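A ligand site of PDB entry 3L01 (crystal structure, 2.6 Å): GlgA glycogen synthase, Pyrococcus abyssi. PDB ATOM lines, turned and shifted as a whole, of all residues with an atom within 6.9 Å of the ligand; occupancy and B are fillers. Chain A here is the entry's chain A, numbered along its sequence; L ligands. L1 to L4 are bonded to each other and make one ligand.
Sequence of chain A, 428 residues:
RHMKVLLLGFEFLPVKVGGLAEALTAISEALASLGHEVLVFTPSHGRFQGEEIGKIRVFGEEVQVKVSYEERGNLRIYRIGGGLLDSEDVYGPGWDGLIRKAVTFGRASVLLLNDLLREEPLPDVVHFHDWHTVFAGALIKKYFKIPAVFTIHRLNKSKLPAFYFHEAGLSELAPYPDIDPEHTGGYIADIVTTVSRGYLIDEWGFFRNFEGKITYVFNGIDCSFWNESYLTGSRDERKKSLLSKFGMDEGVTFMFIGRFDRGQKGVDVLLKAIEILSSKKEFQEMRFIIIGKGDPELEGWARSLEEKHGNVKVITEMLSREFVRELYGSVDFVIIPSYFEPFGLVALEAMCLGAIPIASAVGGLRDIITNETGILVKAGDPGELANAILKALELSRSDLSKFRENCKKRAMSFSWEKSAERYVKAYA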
ATOM      1  N   LYS A 159     -18.390   7.228 -13.779  1.00  0.00           N
ATOM      2  CA  LYS A 159     -19.650   6.490 -13.711  1.00  0.00           C
ATOM      3  C   LYS A 159     -19.671   5.434 -12.654  1.00  0.00           C
ATOM      4  O   LYS A 159     -18.633   4.912 -12.276  1.00  0.00           O
ATOM      5  CB  LYS A 159     -19.949   5.827 -15.032  1.00  0.00           C
ATOM      6  CG  LYS A 159     -20.254   6.828 -16.103  1.00  0.00           C
ATOM      7  CD  LYS A 159     -20.673   6.151 -17.372  1.00  0.00           C
ATOM      8  CE  LYS A 159     -20.859   7.184 -18.474  1.00  0.00           C
ATOM      9  NZ  LYS A 159     -20.933   6.464 -19.763  1.00  0.00           N
ATOM     10  N   PHE A 165     -27.440   2.055  -7.509  1.00  0.00           N
ATOM     11  CA  PHE A 165     -28.706   2.762  -7.545  1.00  0.00           C
ATOM     12  C   PHE A 165     -29.846   1.851  -7.182  1.00  0.00           C
ATOM     13  O   PHE A 165     -30.837   2.278  -6.600  1.00  0.00           O
ATOM     14  CB  PHE A 165     -28.922   3.349  -8.928  1.00  0.00           C
ATOM     15  CG  PHE A 165     -28.038   4.522  -9.213  1.00  0.00           C
ATOM     16  CD1 PHE A 165     -26.835   4.351  -9.864  1.00  0.00           C
ATOM     17  CD2 PHE A 165     -28.395   5.793  -8.765  1.00  0.00           C
ATOM     18  CE1 PHE A 165     -25.994   5.414 -10.103  1.00  0.00           C
ATOM     19  CE2 PHE A 165     -27.562   6.881  -8.987  1.00  0.00           C
ATOM     20  CZ  PHE A 165     -26.347   6.693  -9.652  1.00  0.00           C
ATOM     21  N   LEU A 170     -33.190   3.058  -6.061  1.00  0.00           N
ATOM     22  CA  LEU A 170     -33.369   4.093  -7.072  1.00  0.00           C
ATOM     23  C   LEU A 170     -33.378   3.488  -8.466  1.00  0.00           C
ATOM     24  O   LEU A 170     -32.900   4.084  -9.430  1.00  0.00           O
ATOM     25  CB  LEU A 170     -32.269   5.153  -6.940  1.00  0.00           C
ATOM     26  CG  LEU A 170     -32.425   6.081  -5.720  1.00  0.00           C
ATOM     27  CD1 LEU A 170     -31.195   6.974  -5.486  1.00  0.00           C
ATOM     28  CD2 LEU A 170     -33.665   6.960  -5.848  1.00  0.00           C
ATOM     29  N   SER A 171     -33.902   2.295  -8.576  1.00  0.00           N
ATOM     30  CA  SER A 171     -33.841   1.564  -9.829  1.00  0.00           C
ATOM     31  C   SER A 171     -34.243   2.359 -11.028  1.00  0.00           C
ATOM     32  O   SER A 171     -33.596   2.271 -12.050  1.00  0.00           O
ATOM     33  CB  SER A 171     -34.739   0.374  -9.775  1.00  0.00           C
ATOM     34  OG  SER A 171     -34.013  -0.589  -9.088  1.00  0.00           O
ATOM     35  N   GLU A 172     -35.315   3.121 -10.896  1.00  0.00           N
ATOM     36  CA  GLU A 172     -35.816   3.949 -11.960  1.00  0.00           C
ATOM     37  C   GLU A 172     -34.746   4.914 -12.466  1.00  0.00           C
ATOM     38  O   GLU A 172     -34.846   5.388 -13.579  1.00  0.00           O
ATOM     39  CB  GLU A 172     -37.063   4.703 -11.494  1.00  0.00           C
ATOM     40  CG  GLU A 172     -36.802   5.910 -10.522  1.00  0.00           C
ATOM     41  CD  GLU A 172     -36.571   5.521  -9.056  1.00  0.00           C
ATOM     42  OE1 GLU A 172     -36.579   4.320  -8.724  1.00  0.00           O
ATOM     43  OE2 GLU A 172     -36.359   6.433  -8.215  1.00  0.00           O
ATOM     44  N   LEU A 173     -33.722   5.228 -11.669  1.00  0.00           N
ATOM     45  CA  LEU A 173     -32.670   6.137 -12.119  1.00  0.00           C
ATOM     46  C   LEU A 173     -31.523   5.370 -12.765  1.00  0.00           C
ATOM     47  O   LEU A 173     -30.473   5.925 -13.106  1.00  0.00           O
ATOM     48  CB  LEU A 173     -32.150   6.994 -10.964  1.00  0.00           C
ATOM     49  CG  LEU A 173     -33.218   7.874 -10.288  1.00  0.00           C
ATOM     50  CD1 LEU A 173     -32.663   8.642  -9.121  1.00  0.00           C
ATOM     51  CD2 LEU A 173     -33.837   8.825 -11.305  1.00  0.00           C
ATOM     52  N   ALA A 174     -31.717   4.082 -12.973  1.00  0.00           N
ATOM     53  CA  ALA A 174     -30.634   3.269 -13.462  1.00  0.00           C
ATOM     54  C   ALA A 174     -31.063   2.503 -14.700  1.00  0.00           C
ATOM     55  O   ALA A 174     -31.093   1.302 -14.705  1.00  0.00           O
ATOM     56  CB  ALA A 174     -30.169   2.297 -12.379  1.00  0.00           C
ATOM     57  N   PRO A 175     -31.405   3.206 -15.769  1.00  0.00           N
ATOM     58  CA  PRO A 175     -31.803   2.420 -16.934  1.00  0.00           C
ATOM     59  C   PRO A 175     -30.637   1.919 -17.789  1.00  0.00           C
ATOM     60  O   PRO A 175     -30.885   1.469 -18.879  1.00  0.00           O
ATOM     61  CB  PRO A 175     -32.597   3.419 -17.748  1.00  0.00           C
ATOM     62  CG  PRO A 175     -31.919   4.751 -17.460  1.00  0.00           C
ATOM     63  CD  PRO A 175     -31.426   4.662 -16.034  1.00  0.00           C
ATOM     64  N   TYR A 176     -29.395   2.036 -17.315  1.00  0.00           N
ATOM     65  CA  TYR A 176     -28.248   1.497 -18.054  1.00  0.00           C
ATOM     66  C   TYR A 176     -27.280   0.829 -17.124  1.00  0.00           C
ATOM     67  O   TYR A 176     -27.240   1.123 -15.937  1.00  0.00           O
ATOM     68  CB  TYR A 176     -27.486   2.602 -18.762  1.00  0.00           C
ATOM     69  CG  TYR A 176     -28.336   3.507 -19.555  1.00  0.00           C
ATOM     70  CD1 TYR A 176     -28.473   4.836 -19.192  1.00  0.00           C
ATOM     71  CD2 TYR A 176     -29.011   3.044 -20.664  1.00  0.00           C
ATOM     72  CE1 TYR A 176     -29.255   5.678 -19.927  1.00  0.00           C
ATOM     73  CE2 TYR A 176     -29.792   3.876 -21.409  1.00  0.00           C
ATOM     74  CZ  TYR A 176     -29.911   5.188 -21.031  1.00  0.00           C
ATOM     75  OH  TYR A 176     -30.708   6.001 -21.760  1.00  0.00           O
ATOM     76  N   PRO A 177     -26.420  -0.028 -17.679  1.00  0.00           N
ATOM     77  CA  PRO A 177     -25.501  -0.750 -16.826  1.00  0.00           C
ATOM     78  C   PRO A 177     -24.591   0.178 -16.021  1.00  0.00           C
ATOM     79  O   PRO A 177     -24.087  -0.209 -14.990  1.00  0.00           O
ATOM     80  CB  PRO A 177     -24.705  -1.614 -17.808  1.00  0.00           C
ATOM     81  CG  PRO A 177     -25.546  -1.713 -19.024  1.00  0.00           C
ATOM     82  CD  PRO A 177     -26.300  -0.426 -19.095  1.00  0.00           C
ATOM     83  N   ASP A 178     -24.407   1.399 -16.502  1.00  0.00           N
ATOM     84  CA  ASP A 178     -23.500   2.350 -15.838  1.00  0.00           C
ATOM     85  C   ASP A 178     -24.048   3.749 -15.976  1.00  0.00           C
ATOM     86  O   ASP A 178     -24.551   4.108 -17.038  1.00  0.00           O
ATOM     87  CB  ASP A 178     -22.119   2.345 -16.483  1.00  0.00           C
ATOM     88  CG  ASP A 178     -21.414   1.030 -16.307  1.00  0.00           C
ATOM     89  OD1 ASP A 178     -20.891   0.790 -15.197  1.00  0.00           O
ATOM     90  OD2 ASP A 178     -21.371   0.256 -17.282  1.00  0.00           O
ATOM     91  N   ILE A 179     -23.888   4.525 -14.918  1.00  0.00           N
ATOM     92  CA  ILE A 179     -24.656   5.733 -14.716  1.00  0.00           C
ATOM     93  C   ILE A 179     -23.763   6.778 -14.124  1.00  0.00           C
ATOM     94  O   ILE A 179     -23.078   6.520 -13.168  1.00  0.00           O
ATOM     95  CB  ILE A 179     -25.772   5.487 -13.674  1.00  0.00           C
ATOM     96  CG1 ILE A 179     -26.826   4.528 -14.207  1.00  0.00           C
ATOM     97  CG2 ILE A 179     -26.433   6.789 -13.249  1.00  0.00           C
ATOM     98  CD1 ILE A 179     -27.484   5.004 -15.471  1.00  0.00           C
ATOM     99  N   ASP A 180     -23.762   7.957 -14.718  1.00  0.00           N
ATOM    100  CA  ASP A 180     -23.032   9.078 -14.191  1.00  0.00           C
ATOM    101  C   ASP A 180     -23.844   9.699 -13.076  1.00  0.00           C
ATOM    102  O   ASP A 180     -24.916  10.237 -13.321  1.00  0.00           O
ATOM    103  CB  ASP A 180     -22.830  10.109 -15.301  1.00  0.00           C
ATOM    104  CG  ASP A 180     -22.163  11.375 -14.826  1.00  0.00           C
ATOM    105  OD1 ASP A 180     -22.152  11.679 -13.612  1.00  0.00           O
ATOM    106  OD2 ASP A 180     -21.641  12.098 -15.702  1.00  0.00           O
ATOM    107  N   PRO A 181     -23.328   9.656 -11.837  1.00  0.00           N
ATOM    108  CA  PRO A 181     -24.107  10.143 -10.717  1.00  0.00           C
ATOM    109  C   PRO A 181     -24.319  11.645 -10.741  1.00  0.00           C
ATOM    110  O   PRO A 181     -25.322  12.147 -10.252  1.00  0.00           O
ATOM    111  CB  PRO A 181     -23.283   9.685  -9.499  1.00  0.00           C
ATOM    112  CG  PRO A 181     -21.905   9.598  -9.962  1.00  0.00           C
ATOM    113  CD  PRO A 181     -21.987   9.194 -11.411  1.00  0.00           C
ATOM    114  N   GLU A 182     -23.373  12.388 -11.305  1.00  0.00           N
ATOM    115  CA  GLU A 182     -23.542  13.836 -11.439  1.00  0.00           C
ATOM    116  C   GLU A 182     -24.703  14.122 -12.368  1.00  0.00           C
ATOM    117  O   GLU A 182     -25.538  14.997 -12.107  1.00  0.00           O
ATOM    118  CB  GLU A 182     -22.244  14.457 -11.909  1.00  0.00           C
ATOM    119  CG  GLU A 182     -21.244  14.516 -10.772  1.00  0.00           C
ATOM    120  CD  GLU A 182     -19.806  14.646 -11.223  1.00  0.00           C
ATOM    121  OE1 GLU A 182     -19.486  14.269 -12.377  1.00  0.00           O
ATOM    122  OE2 GLU A 182     -18.971  15.092 -10.417  1.00  0.00           O
ATOM    123  N   HIS A 183     -24.804  13.330 -13.418  1.00  0.00           N
ATOM    124  CA  HIS A 183     -25.864  13.501 -14.383  1.00  0.00           C
ATOM    125  C   HIS A 183     -27.226  13.148 -13.773  1.00  0.00           C
ATOM    126  O   HIS A 183     -28.287  13.751 -14.093  1.00  0.00           O
ATOM    127  CB  HIS A 183     -25.608  12.622 -15.612  1.00  0.00           C
ATOM    128  CG  HIS A 183     -26.395  13.050 -16.812  1.00  0.00           C
ATOM    129  ND1 HIS A 183     -25.878  13.055 -18.088  1.00  0.00           N
ATOM    130  CD2 HIS A 183     -27.667  13.499 -16.915  1.00  0.00           C
ATOM    131  CE1 HIS A 183     -26.793  13.476 -18.934  1.00  0.00           C
ATOM    132  NE2 HIS A 183     -27.893  13.755 -18.249  1.00  0.00           N
ATOM    133  N   THR A 184     -27.230  12.133 -12.919  1.00  0.00           N
ATOM    134  CA  THR A 184     -28.421  11.761 -12.210  1.00  0.00           C
ATOM    135  C   THR A 184     -28.869  12.913 -11.291  1.00  0.00           C
ATOM    136  O   THR A 184     -30.059  13.219 -11.193  1.00  0.00           O
ATOM    137  CB  THR A 184     -28.155  10.541 -11.371  1.00  0.00           C
ATOM    138  OG1 THR A 184     -27.828   9.462 -12.238  1.00  0.00           O
ATOM    139  CG2 THR A 184     -29.352  10.174 -10.555  1.00  0.00           C
ATOM    140  N   GLY A 185     -27.905  13.548 -10.604  1.00  0.00           N
ATOM    141  CA  GLY A 185     -28.227  14.581  -9.642  1.00  0.00           C
ATOM    142  C   GLY A 185     -28.861  15.786 -10.345  1.00  0.00           C
ATOM    143  O   GLY A 185     -29.813  16.387  -9.846  1.00  0.00           O
ATOM    144  N   TYR A 187     -30.277  15.595 -13.108  1.00  0.00           N
ATOM    145  CA  TYR A 187     -31.478  15.124 -13.713  1.00  0.00           C
ATOM    146  C   TYR A 187     -32.710  15.183 -12.808  1.00  0.00           C
ATOM    147  O   TYR A 187     -33.782  15.602 -13.259  1.00  0.00           O
ATOM    148  CB  TYR A 187     -31.293  13.690 -14.151  1.00  0.00           C
ATOM    149  CG  TYR A 187     -32.582  13.099 -14.631  1.00  0.00           C
ATOM    150  CD1 TYR A 187     -33.104  13.458 -15.842  1.00  0.00           C
ATOM    151  CD2 TYR A 187     -33.276  12.176 -13.862  1.00  0.00           C
ATOM    152  CE1 TYR A 187     -34.268  12.907 -16.312  1.00  0.00           C
ATOM    153  CE2 TYR A 187     -34.435  11.629 -14.316  1.00  0.00           C
ATOM    154  CZ  TYR A 187     -34.918  12.007 -15.552  1.00  0.00           C
ATOM    155  OH  TYR A 187     -36.067  11.485 -16.028  1.00  0.00           O
ATOM    156  N   ILE A 188     -32.587  14.737 -11.559  1.00  0.00           N
ATOM    157  CA  ILE A 188     -33.732  14.798 -10.641  1.00  0.00           C
ATOM    158  C   ILE A 188     -33.886  16.180  -9.953  1.00  0.00           C
ATOM    159  O   ILE A 188     -34.912  16.464  -9.351  1.00  0.00           O
ATOM    160  CB  ILE A 188     -33.644  13.689  -9.562  1.00  0.00           C
ATOM    161  CG1 ILE A 188     -32.487  13.941  -8.611  1.00  0.00           C
ATOM    162  CG2 ILE A 188     -33.475  12.354 -10.197  1.00  0.00           C
ATOM    163  CD1 ILE A 188     -32.892  14.630  -7.413  1.00  0.00           C
ATOM    164  N   ASN A 209     -26.900  19.925 -20.538  1.00  0.00           N
ATOM    165  CA  ASN A 209     -27.969  18.955 -20.401  1.00  0.00           C
ATOM    166  C   ASN A 209     -29.094  19.522 -19.562  1.00  0.00           C
ATOM    167  O   ASN A 209     -30.229  19.102 -19.696  1.00  0.00           O
ATOM    168  CB  ASN A 209     -27.453  17.672 -19.795  1.00  0.00           C
ATOM    169  CG  ASN A 209     -26.538  16.936 -20.759  1.00  0.00           C
ATOM    170  OD1 ASN A 209     -25.364  16.757 -20.491  1.00  0.00           O
ATOM    171  ND2 ASN A 209     -27.070  16.569 -21.916  1.00  0.00           N
HETATM  172  C1  LIG L   1     -28.384  -0.302 -24.046  1.00  0.00           C
HETATM  173  C2  LIG L   1     -27.000  -0.709 -23.497  1.00  0.00           C
HETATM  174  C3  LIG L   1     -26.245   0.372 -22.700  1.00  0.00           C
HETATM  175  C4  LIG L   1     -26.307   1.768 -23.306  1.00  0.00           C
HETATM  176  C5  LIG L   1     -27.788   2.029 -23.557  1.00  0.00           C
HETATM  177  C6  LIG L   1     -28.055   3.396 -24.158  1.00  0.00           C
HETATM  178  O1  LIG L   1     -29.489  -0.559 -23.142  1.00  0.00           O
HETATM  179  O2  LIG L   1     -27.133  -1.839 -22.634  1.00  0.00           O
HETATM  180  O3  LIG L   1     -24.887  -0.052 -22.501  1.00  0.00           O
HETATM  181  O4  LIG L   1     -25.803   2.738 -22.351  1.00  0.00           O
HETATM  182  O5  LIG L   1     -28.372   1.066 -24.447  1.00  0.00           O
HETATM  183  O6  LIG L   1     -27.801   3.314 -25.559  1.00  0.00           O
HETATM  184  C1  LG2 L   2     -24.507   3.368 -22.465  1.00  0.00           C
HETATM  185  C2  LG2 L   2     -23.806   3.676 -21.119  1.00  0.00           C
HETATM  186  C3  LG2 L   2     -24.489   4.782 -20.274  1.00  0.00           C
HETATM  187  C4  LG2 L   2     -25.016   5.934 -21.105  1.00  0.00           C
HETATM  188  C5  LG2 L   2     -25.716   5.321 -22.311  1.00  0.00           C
HETATM  189  C6  LG2 L   2     -26.432   6.355 -23.160  1.00  0.00           C
HETATM  190  O1  LG2 L   2     -23.723   2.509 -20.269  1.00  0.00           O
HETATM  191  O2  LG2 L   2     -23.591   5.344 -19.304  1.00  0.00           O
HETATM  192  O3  LG2 L   2     -25.852   6.751 -20.280  1.00  0.00           O
HETATM  193  O4  LG2 L   2     -24.721   4.629 -23.075  1.00  0.00           O
HETATM  194  O5  LG2 L   2     -25.864   7.612 -22.842  1.00  0.00           O
HETATM  195  C1  LG3 L   3     -25.309   8.081 -20.138  1.00  0.00           C
HETATM  196  C2  LG3 L   3     -24.943   8.467 -18.706  1.00  0.00           C
HETATM  197  C3  LG3 L   3     -26.170   8.375 -17.839  1.00  0.00           C
HETATM  198  C4  LG3 L   3     -27.261   9.299 -18.360  1.00  0.00           C
HETATM  199  C5  LG3 L   3     -27.482   9.049 -19.855  1.00  0.00           C
HETATM  200  C6  LG3 L   3     -28.328  10.172 -20.452  1.00  0.00           C
HETATM  201  O1  LG3 L   3     -23.931   7.618 -18.141  1.00  0.00           O
HETATM  202  O2  LG3 L   3     -25.845   8.683 -16.463  1.00  0.00           O
HETATM  203  O3  LG3 L   3     -28.471   9.012 -17.651  1.00  0.00           O
HETATM  204  O4  LG3 L   3     -26.268   9.021 -20.592  1.00  0.00           O
HETATM  205  O5  LG3 L   3     -29.381  10.479 -19.527  1.00  0.00           O
HETATM  206  C1  LG4 L   4     -29.147  10.080 -17.007  1.00  0.00           C
HETATM  207  C2  LG4 L   4     -29.092   9.807 -15.509  1.00  0.00           C
HETATM  208  C3  LG4 L   4     -30.031   8.689 -15.061  1.00  0.00           C
HETATM  209  C4  LG4 L   4     -31.396   8.973 -15.652  1.00  0.00           C
HETATM  210  C5  LG4 L   4     -31.267   9.020 -17.161  1.00  0.00           C
HETATM  211  C6  LG4 L   4     -32.620   9.029 -17.879  1.00  0.00           C
HETATM  212  O1  LG4 L   4     -27.736   9.442 -15.222  1.00  0.00           O
HETATM  213  O2  LG4 L   4     -30.084   8.550 -13.609  1.00  0.00           O
HETATM  214  O3  LG4 L   4     -32.312   7.924 -15.309  1.00  0.00           O
HETATM  215  O4  LG4 L   4     -30.498  10.180 -17.476  1.00  0.00           O
HETATM  216  O5  LG4 L   4     -32.951  10.326 -18.367  1.00  0.00           O
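The backbone carbonyl oxygen (O) of Asp 180 lies within hydrogen-bond range of an oxygen (O1) of LG4 L4. O of Asp 178 is in hydrogen-bond range of O2 of LG2 L2. The backbone NH (N) of Asp 180 sits at hydrogen-bond distance from an oxygen (O2) of LG3 L3, 2.8 Å away. The backbone carbonyl oxygen (O) of Leu 173 is in hydrogen-bond range of an oxygen (O2) of LG4 L4, 2.7 Å away. OG1 of Thr 184 sits at hydrogen-bond distance from O2 of LG4 L4, 2.8 Å away. O2 of LG2 L2 lies within hydrogen-bond range of NZ of Lys 159.
N of Glu 182 lies within hydrogen-bond range of OD1 of Asp 180 (2.7 Å). The side-chain hydroxyl (OG1) of Thr 184 is in hydrogen-bond range of the backbone carbonyl oxygen (O) of Asp 180 (3.2 Å). N of His 183 lies within hydrogen-bond range of OD1 of Asp 180 (3.1 Å).
Residues that only touch the ligand: Tyr 176 (3.3 Å), Pro 175 (3.5 Å), Tyr 187 (3.6 Å), Ile 179 (3.6 Å), Pro 177 (3.7 Å), His 183 (3.7 Å) and Glu 172 (3.98 Å). Hydrophobic or aromatic side chains that line the ligand: Leu 173, Pro 175, Tyr 176, Pro 177, Ile 179, His 183 and Tyr 187. 12 residues have an atom within 4 Å of the ligand: Lys 159, Glu 172, Leu 173, Pro 175, Tyr 176, Pro 177, Asp 178, Ile 179, Asp 180, His 183, Thr 184 and Tyr 187.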
